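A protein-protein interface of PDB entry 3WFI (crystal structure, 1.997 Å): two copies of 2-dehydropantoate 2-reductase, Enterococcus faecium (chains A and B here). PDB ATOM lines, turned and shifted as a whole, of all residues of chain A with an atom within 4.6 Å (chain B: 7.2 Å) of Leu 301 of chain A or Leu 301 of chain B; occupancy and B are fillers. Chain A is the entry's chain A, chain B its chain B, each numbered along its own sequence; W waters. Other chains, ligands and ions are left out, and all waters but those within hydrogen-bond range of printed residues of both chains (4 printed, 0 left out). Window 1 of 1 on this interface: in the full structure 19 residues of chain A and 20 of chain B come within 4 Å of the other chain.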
ATOM      1  N   LEU A 197     -10.196 -17.408  10.090  1.00  0.00           N
ATOM      2  CA  LEU A 197     -10.408 -16.915  11.450  1.00  0.00           C
ATOM      3  C   LEU A 197     -11.619 -16.003  11.553  1.00  0.00           C
ATOM      4  O   LEU A 197     -12.428 -16.142  12.478  1.00  0.00           O
ATOM      5  CB  LEU A 197      -9.138 -16.226  11.982  1.00  0.00           C
ATOM      6  CG  LEU A 197      -7.913 -17.133  12.134  1.00  0.00           C
ATOM      7  CD1 LEU A 197      -6.700 -16.303  12.517  1.00  0.00           C
ATOM      8  CD2 LEU A 197      -8.140 -18.254  13.162  1.00  0.00           C
ATOM      9  N   ILE A 200     -14.874 -18.162  11.055  1.00  0.00           N
ATOM     10  CA  ILE A 200     -15.241 -18.970  12.189  1.00  0.00           C
ATOM     11  C   ILE A 200     -15.632 -18.115  13.409  1.00  0.00           C
ATOM     12  O   ILE A 200     -16.575 -18.453  14.103  1.00  0.00           O
ATOM     13  CB  ILE A 200     -14.113 -19.960  12.566  1.00  0.00           C
ATOM     14  CG1 ILE A 200     -13.895 -20.981  11.446  1.00  0.00           C
ATOM     15  CG2 ILE A 200     -14.452 -20.702  13.843  1.00  0.00           C
ATOM     16  CD1 ILE A 200     -15.057 -21.929  11.244  1.00  0.00           C
ATOM     17  N   LEU A 201     -14.905 -17.025  13.672  1.00  0.00           N
ATOM     18  CA  LEU A 201     -15.167 -16.210  14.859  1.00  0.00           C
ATOM     19  C   LEU A 201     -16.296 -15.182  14.670  1.00  0.00           C
ATOM     20  O   LEU A 201     -16.762 -14.578  15.655  1.00  0.00           O
ATOM     21  CB  LEU A 201     -13.889 -15.510  15.332  1.00  0.00           C
ATOM     22  CG  LEU A 201     -12.820 -16.455  15.876  1.00  0.00           C
ATOM     23  CD1 LEU A 201     -11.478 -15.746  15.972  1.00  0.00           C
ATOM     24  CD2 LEU A 201     -13.248 -17.015  17.229  1.00  0.00           C
ATOM     25  N   MET A 217      -2.496 -17.042  16.955  1.00  0.00           N
ATOM     26  CA  MET A 217      -3.090 -17.906  15.945  1.00  0.00           C
ATOM     27  C   MET A 217      -2.471 -17.609  14.576  1.00  0.00           C
ATOM     28  O   MET A 217      -2.160 -18.529  13.818  1.00  0.00           O
ATOM     29  CB  MET A 217      -4.613 -17.741  15.931  1.00  0.00           C
ATOM     30  CG  MET A 217      -5.265 -18.286  17.193  1.00  0.00           C
ATOM     31  SD  MET A 217      -7.072 -18.203  17.181  1.00  0.00           S
ATOM     32  CE  MET A 217      -7.369 -16.439  17.207  1.00  0.00           C
ATOM     33  N   PHE A 297      -6.989 -28.069  11.265  1.00  0.00           N
ATOM     34  CA  PHE A 297      -8.126 -27.753  12.157  1.00  0.00           C
ATOM     35  C   PHE A 297      -8.997 -26.621  11.593  1.00  0.00           C
ATOM     36  O   PHE A 297     -10.221 -26.712  11.607  1.00  0.00           O
ATOM     37  CB  PHE A 297      -7.588 -27.403  13.553  1.00  0.00           C
ATOM     38  CG  PHE A 297      -8.590 -27.495  14.689  1.00  0.00           C
ATOM     39  CD1 PHE A 297      -8.203 -27.087  15.954  1.00  0.00           C
ATOM     40  CD2 PHE A 297      -9.879 -27.984  14.525  1.00  0.00           C
ATOM     41  CE1 PHE A 297      -9.080 -27.160  17.032  1.00  0.00           C
ATOM     42  CE2 PHE A 297     -10.755 -28.057  15.589  1.00  0.00           C
ATOM     43  CZ  PHE A 297     -10.376 -27.628  16.838  1.00  0.00           C
ATOM     44  N   LEU A 298      -8.355 -25.565  11.082  1.00  0.00           N
ATOM     45  CA  LEU A 298      -9.077 -24.432  10.522  1.00  0.00           C
ATOM     46  C   LEU A 298      -9.874 -24.870   9.299  1.00  0.00           C
ATOM     47  O   LEU A 298     -11.024 -24.487   9.136  1.00  0.00           O
ATOM     48  CB  LEU A 298      -8.127 -23.297  10.182  1.00  0.00           C
ATOM     49  CG  LEU A 298      -8.800 -21.962   9.803  1.00  0.00           C
ATOM     50  CD1 LEU A 298      -9.834 -21.536  10.829  1.00  0.00           C
ATOM     51  CD2 LEU A 298      -7.747 -20.881   9.644  1.00  0.00           C
ATOM     52  N   THR A 299      -9.272 -25.716   8.471  1.00  0.00           N
ATOM     53  CA  THR A 299      -9.963 -26.287   7.333  1.00  0.00           C
ATOM     54  C   THR A 299     -11.173 -27.114   7.779  1.00  0.00           C
ATOM     55  O   THR A 299     -12.285 -26.961   7.240  1.00  0.00           O
ATOM     56  CB  THR A 299      -9.009 -27.133   6.481  1.00  0.00           C
ATOM     57  OG1 THR A 299      -7.968 -26.282   5.993  1.00  0.00           O
ATOM     58  CG2 THR A 299      -9.740 -27.763   5.294  1.00  0.00           C
ATOM     59  N   GLU A 300     -10.951 -27.978   8.755  1.00  0.00           N
ATOM     60  CA  GLU A 300     -12.009 -28.810   9.333  1.00  0.00           C
ATOM     61  C   GLU A 300     -13.145 -27.972   9.925  1.00  0.00           C
ATOM     62  O   GLU A 300     -14.317 -28.268   9.692  1.00  0.00           O
ATOM     63  CB  GLU A 300     -11.416 -29.755  10.373  1.00  0.00           C
ATOM     64  CG  GLU A 300     -10.612 -30.892   9.761  1.00  0.00           C
ATOM     65  CD  GLU A 300      -9.504 -31.385  10.673  1.00  0.00           C
ATOM     66  OE1 GLU A 300      -9.520 -31.060  11.875  1.00  0.00           O
ATOM     67  OE2 GLU A 300      -8.610 -32.088  10.163  1.00  0.00           O
ATOM     68  N   LEU A 301     -12.794 -26.891  10.617  1.00  0.00           N
ATOM     69  CA  LEU A 301     -13.785 -25.994  11.192  1.00  0.00           C
ATOM     70  C   LEU A 301     -14.615 -25.282  10.133  1.00  0.00           C
ATOM     71  O   LEU A 301     -15.823 -25.136  10.284  1.00  0.00           O
ATOM     72  CB  LEU A 301     -13.117 -24.966  12.127  1.00  0.00           C
ATOM     73  CG  LEU A 301     -12.628 -25.530  13.455  1.00  0.00           C
ATOM     74  CD1 LEU A 301     -11.657 -24.571  14.128  1.00  0.00           C
ATOM     75  CD2 LEU A 301     -13.807 -25.842  14.369  1.00  0.00           C
ATOM     76  N   VAL A 302     -13.960 -24.797   9.081  1.00  0.00           N
ATOM     77  CA  VAL A 302     -14.656 -24.047   8.056  1.00  0.00           C
ATOM     78  C   VAL A 302     -15.613 -24.992   7.313  1.00  0.00           C
ATOM     79  O   VAL A 302     -16.744 -24.624   7.026  1.00  0.00           O
ATOM     80  CB  VAL A 302     -13.680 -23.350   7.085  1.00  0.00           C
ATOM     81  CG1 VAL A 302     -14.405 -22.820   5.858  1.00  0.00           C
ATOM     82  CG2 VAL A 302     -12.951 -22.209   7.799  1.00  0.00           C
ATOM     83  N   HIS A 303     -15.169 -26.206   7.033  1.00  0.00           N
ATOM     84  CA  HIS A 303     -16.065 -27.206   6.453  1.00  0.00           C
ATOM     85  C   HIS A 303     -17.261 -27.539   7.331  1.00  0.00           C
ATOM     86  O   HIS A 303     -18.387 -27.652   6.827  1.00  0.00           O
ATOM     87  CB  HIS A 303     -15.308 -28.472   6.083  1.00  0.00           C
ATOM     88  CG  HIS A 303     -14.525 -28.319   4.824  1.00  0.00           C
ATOM     89  ND1 HIS A 303     -13.300 -28.915   4.632  1.00  0.00           N
ATOM     90  CD2 HIS A 303     -14.777 -27.602   3.704  1.00  0.00           C
ATOM     91  CE1 HIS A 303     -12.845 -28.595   3.440  1.00  0.00           C
ATOM     92  NE2 HIS A 303     -13.722 -27.798   2.858  1.00  0.00           N
ATOM     93  N   ALA A 304     -17.023 -27.662   8.628  1.00  0.00           N
ATOM     94  CA  ALA A 304     -18.104 -27.891   9.578  1.00  0.00           C
ATOM     95  C   ALA A 304     -19.089 -26.730   9.557  1.00  0.00           C
ATOM     96  O   ALA A 304     -20.310 -26.940   9.656  1.00  0.00           O
ATOM     97  CB  ALA A 304     -17.553 -28.119  10.986  1.00  0.00           C
ATOM     98  N   LYS A 305     -18.569 -25.510   9.425  1.00  0.00           N
ATOM     99  CA  LYS A 305     -19.429 -24.324   9.425  1.00  0.00           C
ATOM    100  C   LYS A 305     -20.258 -24.305   8.147  1.00  0.00           C
ATOM    101  O   LYS A 305     -21.454 -24.005   8.196  1.00  0.00           O
ATOM    102  CB  LYS A 305     -18.595 -23.044   9.572  1.00  0.00           C
ATOM    103  CG  LYS A 305     -19.385 -21.745   9.751  1.00  0.00           C
ATOM    104  CD  LYS A 305     -20.132 -21.687  11.070  1.00  0.00           C
ATOM    105  CE  LYS A 305     -20.807 -20.340  11.247  1.00  0.00           C
ATOM    106  NZ  LYS A 305     -21.414 -20.211  12.597  1.00  0.00           N
ATOM    107  N   GLY B 196     -16.090 -26.642  23.516  1.00  0.00           N
ATOM    108  CA  GLY B 196     -15.381 -25.722  22.620  1.00  0.00           C
ATOM    109  C   GLY B 196     -15.895 -25.683  21.198  1.00  0.00           C
ATOM    110  O   GLY B 196     -16.080 -24.594  20.634  1.00  0.00           O
ATOM    111  N   LEU B 197     -16.129 -26.858  20.611  1.00  0.00           N
ATOM    112  CA  LEU B 197     -16.579 -26.943  19.214  1.00  0.00           C
ATOM    113  C   LEU B 197     -17.954 -26.343  19.018  1.00  0.00           C
ATOM    114  O   LEU B 197     -18.178 -25.603  18.056  1.00  0.00           O
ATOM    115  CB  LEU B 197     -16.550 -28.399  18.709  1.00  0.00           C
ATOM    116  CG  LEU B 197     -15.170 -29.041  18.641  1.00  0.00           C
ATOM    117  CD1 LEU B 197     -15.275 -30.518  18.313  1.00  0.00           C
ATOM    118  CD2 LEU B 197     -14.242 -28.328  17.646  1.00  0.00           C
ATOM    119  N   THR B 199     -19.398 -24.117  20.976  1.00  0.00           N
ATOM    120  CA  THR B 199     -19.252 -22.702  21.279  1.00  0.00           C
ATOM    121  C   THR B 199     -18.710 -21.926  20.083  1.00  0.00           C
ATOM    122  O   THR B 199     -19.267 -20.892  19.704  1.00  0.00           O
ATOM    123  CB  THR B 199     -18.345 -22.495  22.502  1.00  0.00           C
ATOM    124  OG1 THR B 199     -18.969 -23.089  23.648  1.00  0.00           O
ATOM    125  CG2 THR B 199     -18.130 -21.019  22.768  1.00  0.00           C
ATOM    126  N   ILE B 200     -17.677 -22.457  19.445  1.00  0.00           N
ATOM    127  CA  ILE B 200     -17.074 -21.780  18.294  1.00  0.00           C
ATOM    128  C   ILE B 200     -17.931 -21.864  17.024  1.00  0.00           C
ATOM    129  O   ILE B 200     -18.046 -20.884  16.301  1.00  0.00           O
ATOM    130  CB  ILE B 200     -15.653 -22.317  17.998  1.00  0.00           C
ATOM    131  CG1 ILE B 200     -14.728 -21.968  19.147  1.00  0.00           C
ATOM    132  CG2 ILE B 200     -15.086 -21.710  16.730  1.00  0.00           C
ATOM    133  CD1 ILE B 200     -14.482 -20.493  19.292  1.00  0.00           C
ATOM    134  N   LEU B 201     -18.518 -23.019  16.756  1.00  0.00           N
ATOM    135  CA  LEU B 201     -19.308 -23.202  15.520  1.00  0.00           C
ATOM    136  C   LEU B 201     -20.752 -22.705  15.623  1.00  0.00           C
ATOM    137  O   LEU B 201     -21.442 -22.594  14.601  1.00  0.00           O
ATOM    138  CB  LEU B 201     -19.282 -24.666  15.091  1.00  0.00           C
ATOM    139  CG  LEU B 201     -17.917 -25.174  14.630  1.00  0.00           C
ATOM    140  CD1 LEU B 201     -17.868 -26.695  14.578  1.00  0.00           C
ATOM    141  CD2 LEU B 201     -17.566 -24.573  13.274  1.00  0.00           C
ATOM    142  N   LEU B 208     -23.539 -30.292  15.553  1.00  0.00           N
ATOM    143  CA  LEU B 208     -22.112 -30.572  15.422  1.00  0.00           C
ATOM    144  C   LEU B 208     -21.910 -31.954  14.783  1.00  0.00           C
ATOM    145  O   LEU B 208     -21.132 -32.109  13.826  1.00  0.00           O
ATOM    146  CB  LEU B 208     -21.428 -30.491  16.788  1.00  0.00           C
ATOM    147  CG  LEU B 208     -19.968 -30.919  16.853  1.00  0.00           C
ATOM    148  CD1 LEU B 208     -19.090 -30.058  15.952  1.00  0.00           C
ATOM    149  CD2 LEU B 208     -19.498 -30.873  18.296  1.00  0.00           C
ATOM    150  N   THR B 213     -16.803 -33.102   9.333  1.00  0.00           N
ATOM    151  CA  THR B 213     -15.487 -33.105  10.002  1.00  0.00           C
ATOM    152  C   THR B 213     -15.525 -33.274  11.526  1.00  0.00           C
ATOM    153  O   THR B 213     -14.469 -33.311  12.176  1.00  0.00           O
ATOM    154  CB  THR B 213     -14.710 -31.807   9.673  1.00  0.00           C
ATOM    155  OG1 THR B 213     -15.506 -30.663   9.998  1.00  0.00           O
ATOM    156  CG2 THR B 213     -14.316 -31.777   8.184  1.00  0.00           C
ATOM    157  N   MET B 217     -12.323 -33.952  14.116  1.00  0.00           N
ATOM    158  CA  MET B 217     -11.935 -32.965  15.139  1.00  0.00           C
ATOM    159  C   MET B 217     -11.981 -33.590  16.540  1.00  0.00           C
ATOM    160  O   MET B 217     -11.074 -33.403  17.348  1.00  0.00           O
ATOM    161  CB  MET B 217     -12.835 -31.737  15.052  1.00  0.00           C
ATOM    162  CG  MET B 217     -12.606 -30.937  13.777  1.00  0.00           C
ATOM    163  SD  MET B 217     -13.528 -29.384  13.690  1.00  0.00           S
ATOM    164  CE  MET B 217     -15.217 -30.006  13.544  1.00  0.00           C
ATOM    165  N   LEU B 265     -20.887 -18.719  27.597  1.00  0.00           N
ATOM    166  CA  LEU B 265     -20.390 -17.651  26.742  1.00  0.00           C
ATOM    167  C   LEU B 265     -21.482 -17.008  25.892  1.00  0.00           C
ATOM    168  O   LEU B 265     -21.703 -15.807  25.978  1.00  0.00           O
ATOM    169  CB  LEU B 265     -19.270 -18.163  25.832  1.00  0.00           C
ATOM    170  CG  LEU B 265     -18.593 -17.109  24.939  1.00  0.00           C
ATOM    171  CD1 LEU B 265     -18.206 -15.878  25.733  1.00  0.00           C
ATOM    172  CD2 LEU B 265     -17.370 -17.703  24.252  1.00  0.00           C
ATOM    173  N   ILE B 274     -12.521 -22.815  29.704  1.00  0.00           N
ATOM    174  CA  ILE B 274     -11.665 -23.429  28.684  1.00  0.00           C
ATOM    175  C   ILE B 274     -10.224 -23.683  29.188  1.00  0.00           C
ATOM    176  O   ILE B 274      -9.624 -24.722  28.866  1.00  0.00           O
ATOM    177  CB  ILE B 274     -11.693 -22.619  27.364  1.00  0.00           C
ATOM    178  CG1 ILE B 274     -11.043 -23.394  26.219  1.00  0.00           C
ATOM    179  CG2 ILE B 274     -11.023 -21.270  27.534  1.00  0.00           C
ATOM    180  CD1 ILE B 274     -11.838 -24.576  25.723  1.00  0.00           C
ATOM    181  N   TYR B 294      -4.434 -28.978  18.696  1.00  0.00           N
ATOM    182  CA  TYR B 294      -5.885 -28.755  18.643  1.00  0.00           C
ATOM    183  C   TYR B 294      -6.382 -28.172  19.974  1.00  0.00           C
ATOM    184  O   TYR B 294      -7.202 -27.274  19.986  1.00  0.00           O
ATOM    185  CB  TYR B 294      -6.663 -30.039  18.269  1.00  0.00           C
ATOM    186  CG  TYR B 294      -6.760 -30.326  16.772  1.00  0.00           C
ATOM    187  CD1 TYR B 294      -5.673 -30.160  15.922  1.00  0.00           C
ATOM    188  CD2 TYR B 294      -7.958 -30.761  16.217  1.00  0.00           C
ATOM    189  CE1 TYR B 294      -5.772 -30.443  14.576  1.00  0.00           C
ATOM    190  CE2 TYR B 294      -8.079 -31.037  14.870  1.00  0.00           C
ATOM    191  CZ  TYR B 294      -6.981 -30.874  14.049  1.00  0.00           C
ATOM    192  OH  TYR B 294      -7.074 -31.147  12.708  1.00  0.00           O
ATOM    193  N   CYS B 295      -5.860 -28.658  21.096  1.00  0.00           N
ATOM    194  CA  CYS B 295      -6.208 -28.083  22.408  1.00  0.00           C
ATOM    195  C   CYS B 295      -5.712 -26.643  22.507  1.00  0.00           C
ATOM    196  O   CYS B 295      -6.430 -25.772  23.011  1.00  0.00           O
ATOM    197  CB  CYS B 295      -5.652 -28.933  23.564  1.00  0.00           C
ATOM    198  SG  CYS B 295      -6.498 -30.507  23.861  1.00  0.00           S
ATOM    199  N   ASP B 296      -4.506 -26.385  22.001  1.00  0.00           N
ATOM    200  CA  ASP B 296      -3.960 -25.006  21.944  1.00  0.00           C
ATOM    201  C   ASP B 296      -4.892 -24.082  21.129  1.00  0.00           C
ATOM    202  O   ASP B 296      -5.301 -23.016  21.588  1.00  0.00           O
ATOM    203  CB  ASP B 296      -2.574 -24.997  21.304  1.00  0.00           C
ATOM    204  CG  ASP B 296      -1.514 -25.770  22.114  1.00  0.00           C
ATOM    205  OD1 ASP B 296      -1.793 -26.294  23.227  1.00  0.00           O
ATOM    206  OD2 ASP B 296      -0.383 -25.887  21.594  1.00  0.00           O
ATOM    207  N   PHE B 297      -5.209 -24.514  19.916  1.00  0.00           N
ATOM    208  CA  PHE B 297      -5.998 -23.713  18.952  1.00  0.00           C
ATOM    209  C   PHE B 297      -7.437 -23.501  19.424  1.00  0.00           C
ATOM    210  O   PHE B 297      -7.958 -22.387  19.350  1.00  0.00           O
ATOM    211  CB  PHE B 297      -5.977 -24.405  17.585  1.00  0.00           C
ATOM    212  CG  PHE B 297      -6.326 -23.521  16.405  1.00  0.00           C
ATOM    213  CD1 PHE B 297      -6.444 -24.094  15.148  1.00  0.00           C
ATOM    214  CD2 PHE B 297      -6.489 -22.139  16.515  1.00  0.00           C
ATOM    215  CE1 PHE B 297      -6.747 -23.335  14.041  1.00  0.00           C
ATOM    216  CE2 PHE B 297      -6.800 -21.377  15.405  1.00  0.00           C
ATOM    217  CZ  PHE B 297      -6.931 -21.969  14.164  1.00  0.00           C
ATOM    218  N   LEU B 298      -8.071 -24.557  19.915  1.00  0.00           N
ATOM    219  CA  LEU B 298      -9.434 -24.453  20.405  1.00  0.00           C
ATOM    220  C   LEU B 298      -9.494 -23.477  21.585  1.00  0.00           C
ATOM    221  O   LEU B 298     -10.415 -22.672  21.685  1.00  0.00           O
ATOM    222  CB  LEU B 298      -9.990 -25.827  20.801  1.00  0.00           C
ATOM    223  CG  LEU B 298     -11.491 -25.876  21.106  1.00  0.00           C
ATOM    224  CD1 LEU B 298     -12.315 -25.212  20.010  1.00  0.00           C
ATOM    225  CD2 LEU B 298     -11.957 -27.307  21.303  1.00  0.00           C
ATOM    226  N   THR B 299      -8.498 -23.559  22.475  1.00  0.00           N
ATOM    227  CA  THR B 299      -8.426 -22.649  23.598  1.00  0.00           C
ATOM    228  C   THR B 299      -8.269 -21.213  23.105  1.00  0.00           C
ATOM    229  O   THR B 299      -8.974 -20.300  23.549  1.00  0.00           O
ATOM    230  CB  THR B 299      -7.274 -23.043  24.542  1.00  0.00           C
ATOM    231  OG1 THR B 299      -7.530 -24.358  25.060  1.00  0.00           O
ATOM    232  CG2 THR B 299      -7.147 -22.069  25.692  1.00  0.00           C
ATOM    233  N   GLU B 300      -7.342 -21.017  22.175  1.00  0.00           N
ATOM    234  CA  GLU B 300      -7.125 -19.704  21.587  1.00  0.00           C
ATOM    235  C   GLU B 300      -8.407 -19.170  20.913  1.00  0.00           C
ATOM    236  O   GLU B 300      -8.731 -17.988  21.040  1.00  0.00           O
ATOM    237  CB  GLU B 300      -5.971 -19.780  20.595  1.00  0.00           C
ATOM    238  CG  GLU B 300      -4.613 -19.885  21.285  1.00  0.00           C
ATOM    239  CD  GLU B 300      -3.592 -20.633  20.472  1.00  0.00           C
ATOM    240  OE1 GLU B 300      -3.813 -20.828  19.250  1.00  0.00           O
ATOM    241  OE2 GLU B 300      -2.578 -21.045  21.066  1.00  0.00           O
ATOM    242  N   LEU B 301      -9.122 -20.040  20.197  1.00  0.00           N
ATOM    243  CA  LEU B 301     -10.341 -19.624  19.510  1.00  0.00           C
ATOM    244  C   LEU B 301     -11.464 -19.233  20.472  1.00  0.00           C
ATOM    245  O   LEU B 301     -12.157 -18.220  20.254  1.00  0.00           O
ATOM    246  CB  LEU B 301     -10.835 -20.731  18.584  1.00  0.00           C
ATOM    247  CG  LEU B 301     -10.031 -20.914  17.310  1.00  0.00           C
ATOM    248  CD1 LEU B 301     -10.360 -22.265  16.671  1.00  0.00           C
ATOM    249  CD2 LEU B 301     -10.294 -19.763  16.353  1.00  0.00           C
ATOM    250  N   VAL B 302     -11.629 -20.001  21.539  1.00  0.00           N
ATOM    251  CA  VAL B 302     -12.669 -19.702  22.526  1.00  0.00           C
ATOM    252  C   VAL B 302     -12.365 -18.377  23.199  1.00  0.00           C
ATOM    253  O   VAL B 302     -13.259 -17.553  23.394  1.00  0.00           O
ATOM    254  CB  VAL B 302     -12.841 -20.842  23.538  1.00  0.00           C
ATOM    255  CG1 VAL B 302     -13.723 -20.423  24.701  1.00  0.00           C
ATOM    256  CG2 VAL B 302     -13.430 -22.060  22.850  1.00  0.00           C
ATOM    257  N   HIS B 303     -11.093 -18.146  23.530  1.00  0.00           N
ATOM    258  CA  HIS B 303     -10.715 -16.851  24.099  1.00  0.00           C
ATOM    259  C   HIS B 303     -10.973 -15.691  23.144  1.00  0.00           C
ATOM    260  O   HIS B 303     -11.444 -14.627  23.566  1.00  0.00           O
ATOM    261  CB  HIS B 303      -9.250 -16.872  24.569  1.00  0.00           C
ATOM    262  CG  HIS B 303      -9.029 -17.603  25.848  1.00  0.00           C
ATOM    263  ND1 HIS B 303      -9.869 -17.489  26.944  1.00  0.00           N
ATOM    264  CD2 HIS B 303      -8.048 -18.457  26.217  1.00  0.00           C
ATOM    265  CE1 HIS B 303      -9.413 -18.251  27.918  1.00  0.00           C
ATOM    266  NE2 HIS B 303      -8.310 -18.843  27.503  1.00  0.00           N
ATOM    267  N   ALA B 304     -10.641 -15.877  21.865  1.00  0.00           N
ATOM    268  CA  ALA B 304     -10.917 -14.863  20.855  1.00  0.00           C
ATOM    269  C   ALA B 304     -12.425 -14.578  20.747  1.00  0.00           C
ATOM    270  O   ALA B 304     -12.837 -13.425  20.552  1.00  0.00           O
ATOM    271  CB  ALA B 304     -10.357 -15.280  19.502  1.00  0.00           C
ATOM    272  N   LYS B 305     -13.237 -15.624  20.888  1.00  0.00           N
ATOM    273  CA  LYS B 305     -14.693 -15.465  20.794  1.00  0.00           C
ATOM    274  C   LYS B 305     -15.214 -14.702  22.023  1.00  0.00           C
ATOM    275  O   LYS B 305     -16.039 -13.796  21.883  1.00  0.00           O
ATOM    276  CB  LYS B 305     -15.386 -16.820  20.689  1.00  0.00           C
ATOM    277  CG  LYS B 305     -16.905 -16.752  20.452  1.00  0.00           C
ATOM    278  CD  LYS B 305     -17.264 -16.188  19.084  1.00  0.00           C
ATOM    279  CE  LYS B 305     -18.769 -16.232  18.846  1.00  0.00           C
ATOM    280  NZ  LYS B 305     -19.122 -15.785  17.481  1.00  0.00           N
ATOM    281  N   GLU B 306     -14.709 -15.063  23.203  1.00  0.00           N
ATOM    282  CA  GLU B 306     -14.946 -14.291  24.436  1.00  0.00           C
ATOM    283  C   GLU B 306     -14.631 -12.813  24.195  1.00  0.00           C
ATOM    284  O   GLU B 306     -15.453 -11.938  24.445  1.00  0.00           O
ATOM    285  CB  GLU B 306     -14.090 -14.818  25.602  1.00  0.00           C
ATOM    286  CG  GLU B 306     -14.504 -16.175  26.155  1.00  0.00           C
ATOM    287  CD  GLU B 306     -13.463 -16.771  27.091  1.00  0.00           C
ATOM    288  OE1 GLU B 306     -12.315 -16.284  27.088  1.00  0.00           O
ATOM    289  OE2 GLU B 306     -13.802 -17.710  27.847  1.00  0.00           O
ATOM    290  N   ASP B 307     -13.435 -12.550  23.691  1.00  0.00           N
ATOM    291  CA  ASP B 307     -12.985 -11.193  23.459  1.00  0.00           C
ATOM    292  C   ASP B 307     -13.910 -10.464  22.484  1.00  0.00           C
ATOM    293  O   ASP B 307     -14.274  -9.325  22.722  1.00  0.00           O
ATOM    294  CB  ASP B 307     -11.549 -11.173  22.942  1.00  0.00           C
ATOM    295  CG  ASP B 307     -10.538 -11.686  23.973  1.00  0.00           C
ATOM    296  OD1 ASP B 307     -10.841 -11.691  25.181  1.00  0.00           O
ATOM    297  OD2 ASP B 307      -9.411 -12.048  23.575  1.00  0.00           O
ATOM    298  N   SER B 308     -14.307 -11.141  21.414  1.00  0.00           N
ATOM    299  CA  SER B 308     -15.156 -10.534  20.396  1.00  0.00           C
ATOM    300  C   SER B 308     -16.544 -10.162  20.924  1.00  0.00           C
ATOM    301  O   SER B 308     -17.195  -9.278  20.368  1.00  0.00           O
ATOM    302  CB  SER B 308     -15.287 -11.453  19.173  1.00  0.00           C
ATOM    303  OG  SER B 308     -16.217 -12.499  19.379  1.00  0.00           O
HETATM  304  O   HOH W   1     -17.996 -13.024  17.494  1.00  0.00           O
HETATM  305  O   HOH W   2     -18.719 -20.070  13.778  1.00  0.00           O
HETATM  306  O   HOH W   3     -23.190 -22.529  12.582  1.00  0.00           O
HETATM  307  O   HOH W   4     -18.420 -17.875  16.010  1.00  0.00           O
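Leu 301 of chain A touches just these residues of chain B: Leu 201, Met 217 and Leu 301. Of chain A, only Leu 201 (3.4 Å), Met 217 (3.7 Å) and Leu 301 (3.7 Å) come within 4 Å of Leu 301 of chain B. Printed residues of chain B within 4 Å of Ala 304 of chain A: Leu 201, Thr 213 and Met 217. Printed residues of chain A within 4 Å of Lys 305 of chain B: Leu 201 (3.2 Å). The nearest residue of chain B that does not touch Leu 301 of chain A is Leu 197 of chain B (4.1 Å). The nearest residue of chain A that does not touch Leu 301 of chain B is Leu 197 of chain A (4.1 Å). The nearest printed residue of chain A that does not touch Lys 305 of chain B is Ile 200 of chain A (5.0 Å).
Met 217 of chain A touches Glu 300 of chain B, and with the chains exchanged Glu 300 of chain A touches Met 217 of chain B. Met 217 of chain A touches Ala 304 of chain B, and with the chains exchanged Ala 304 of chain A touches Met 217 of chain B.
Among the printed residues, merely in contact across the chains: Ile 200 of chain A with Ile 200 of chain B (3.1 Å), Ala 304 of chain A with Thr 213 of chain B (3.4 Å), Leu 201 of chain A with Leu 301 of chain B (3.4 Å), Leu 301 of chain A with Leu 201 of chain B (3.5 Å), Phe 297 of chain A with Phe 297 of chain B (3.6 Å), Met 217 of chain A with Glu 300 of chain B (3.6 Å), Phe 297 of chain A with Met 217 of chain B (3.6 Å), Leu 301 of chain A with Met 217 of chain B (3.6 Å), Glu 300 of chain A with Met 217 of chain B (3.6 Å), Met 217 of chain A with Phe 297 of chain B (3.6 Å), Leu 301 of chain A with Leu 301 of chain B (3.7 Å), Met 217 of chain A with Leu 301 of chain B (3.7 Å), Leu 201 of chain A with Ala 304 of chain B (3.7 Å), Ala 304 of chain A with Leu 201 of chain B (3.9 Å), Met 217 of chain A with Ala 304 of chain B (3.9 Å) and Ala 304 of chain A with Met 217 of chain B (3.9 Å).
Water W1 lies within hydrogen-bond range of OG of Ser 308 of chain B (2.6 Å), O of Leu 201 of chain A (2.7 Å) and NZ of Lys 305 of chain B (3.0 Å).
Of the 13 printed residues of chain A, 8 touch a printed residue of chain B. Hydrophobic or aromatic side chains of chain A within 4 Å of the printed part of chain B: Ile 200, Leu 201, Met 217, Phe 297, Leu 301 and Ala 304. Among the printed residues, 21 pairs touch across the chains. Among the printed residues, no Asp or Glu carboxylate lies within 4 Å of a Lys or Arg side-chain nitrogen of the other chain.
O of Lys 305 of chain B lies within hydrogen-bond range of OG of Ser 308 of chain B, at 2.8 Å.
O of Leu 201 of chain A lies within hydrogen-bond range of NZ of Lys 305 of chain B, at 3.2 Å. The side-chain hydroxyl (OH) of Tyr 294 of chain B lies within hydrogen-bond range of the backbone NH (N) of Phe 297 of chain A. The backbone carbonyl oxygen (O) of Glu 300 of chain A is in hydrogen-bond range of the side-chain hydroxyl (OG1) of Thr 213 of chain B (2.7 Å). The side-chain carboxylate of Glu 300 of chain A sits at hydrogen-bond distance from the side-chain hydroxyl of Tyr 294 of chain B, at 2.6 Å. The side-chain amino group of Lys 305 of chain A lies within hydrogen-bond range of the backbone carbonyl oxygen of Leu 201 of chain B, 3.1 Å away.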
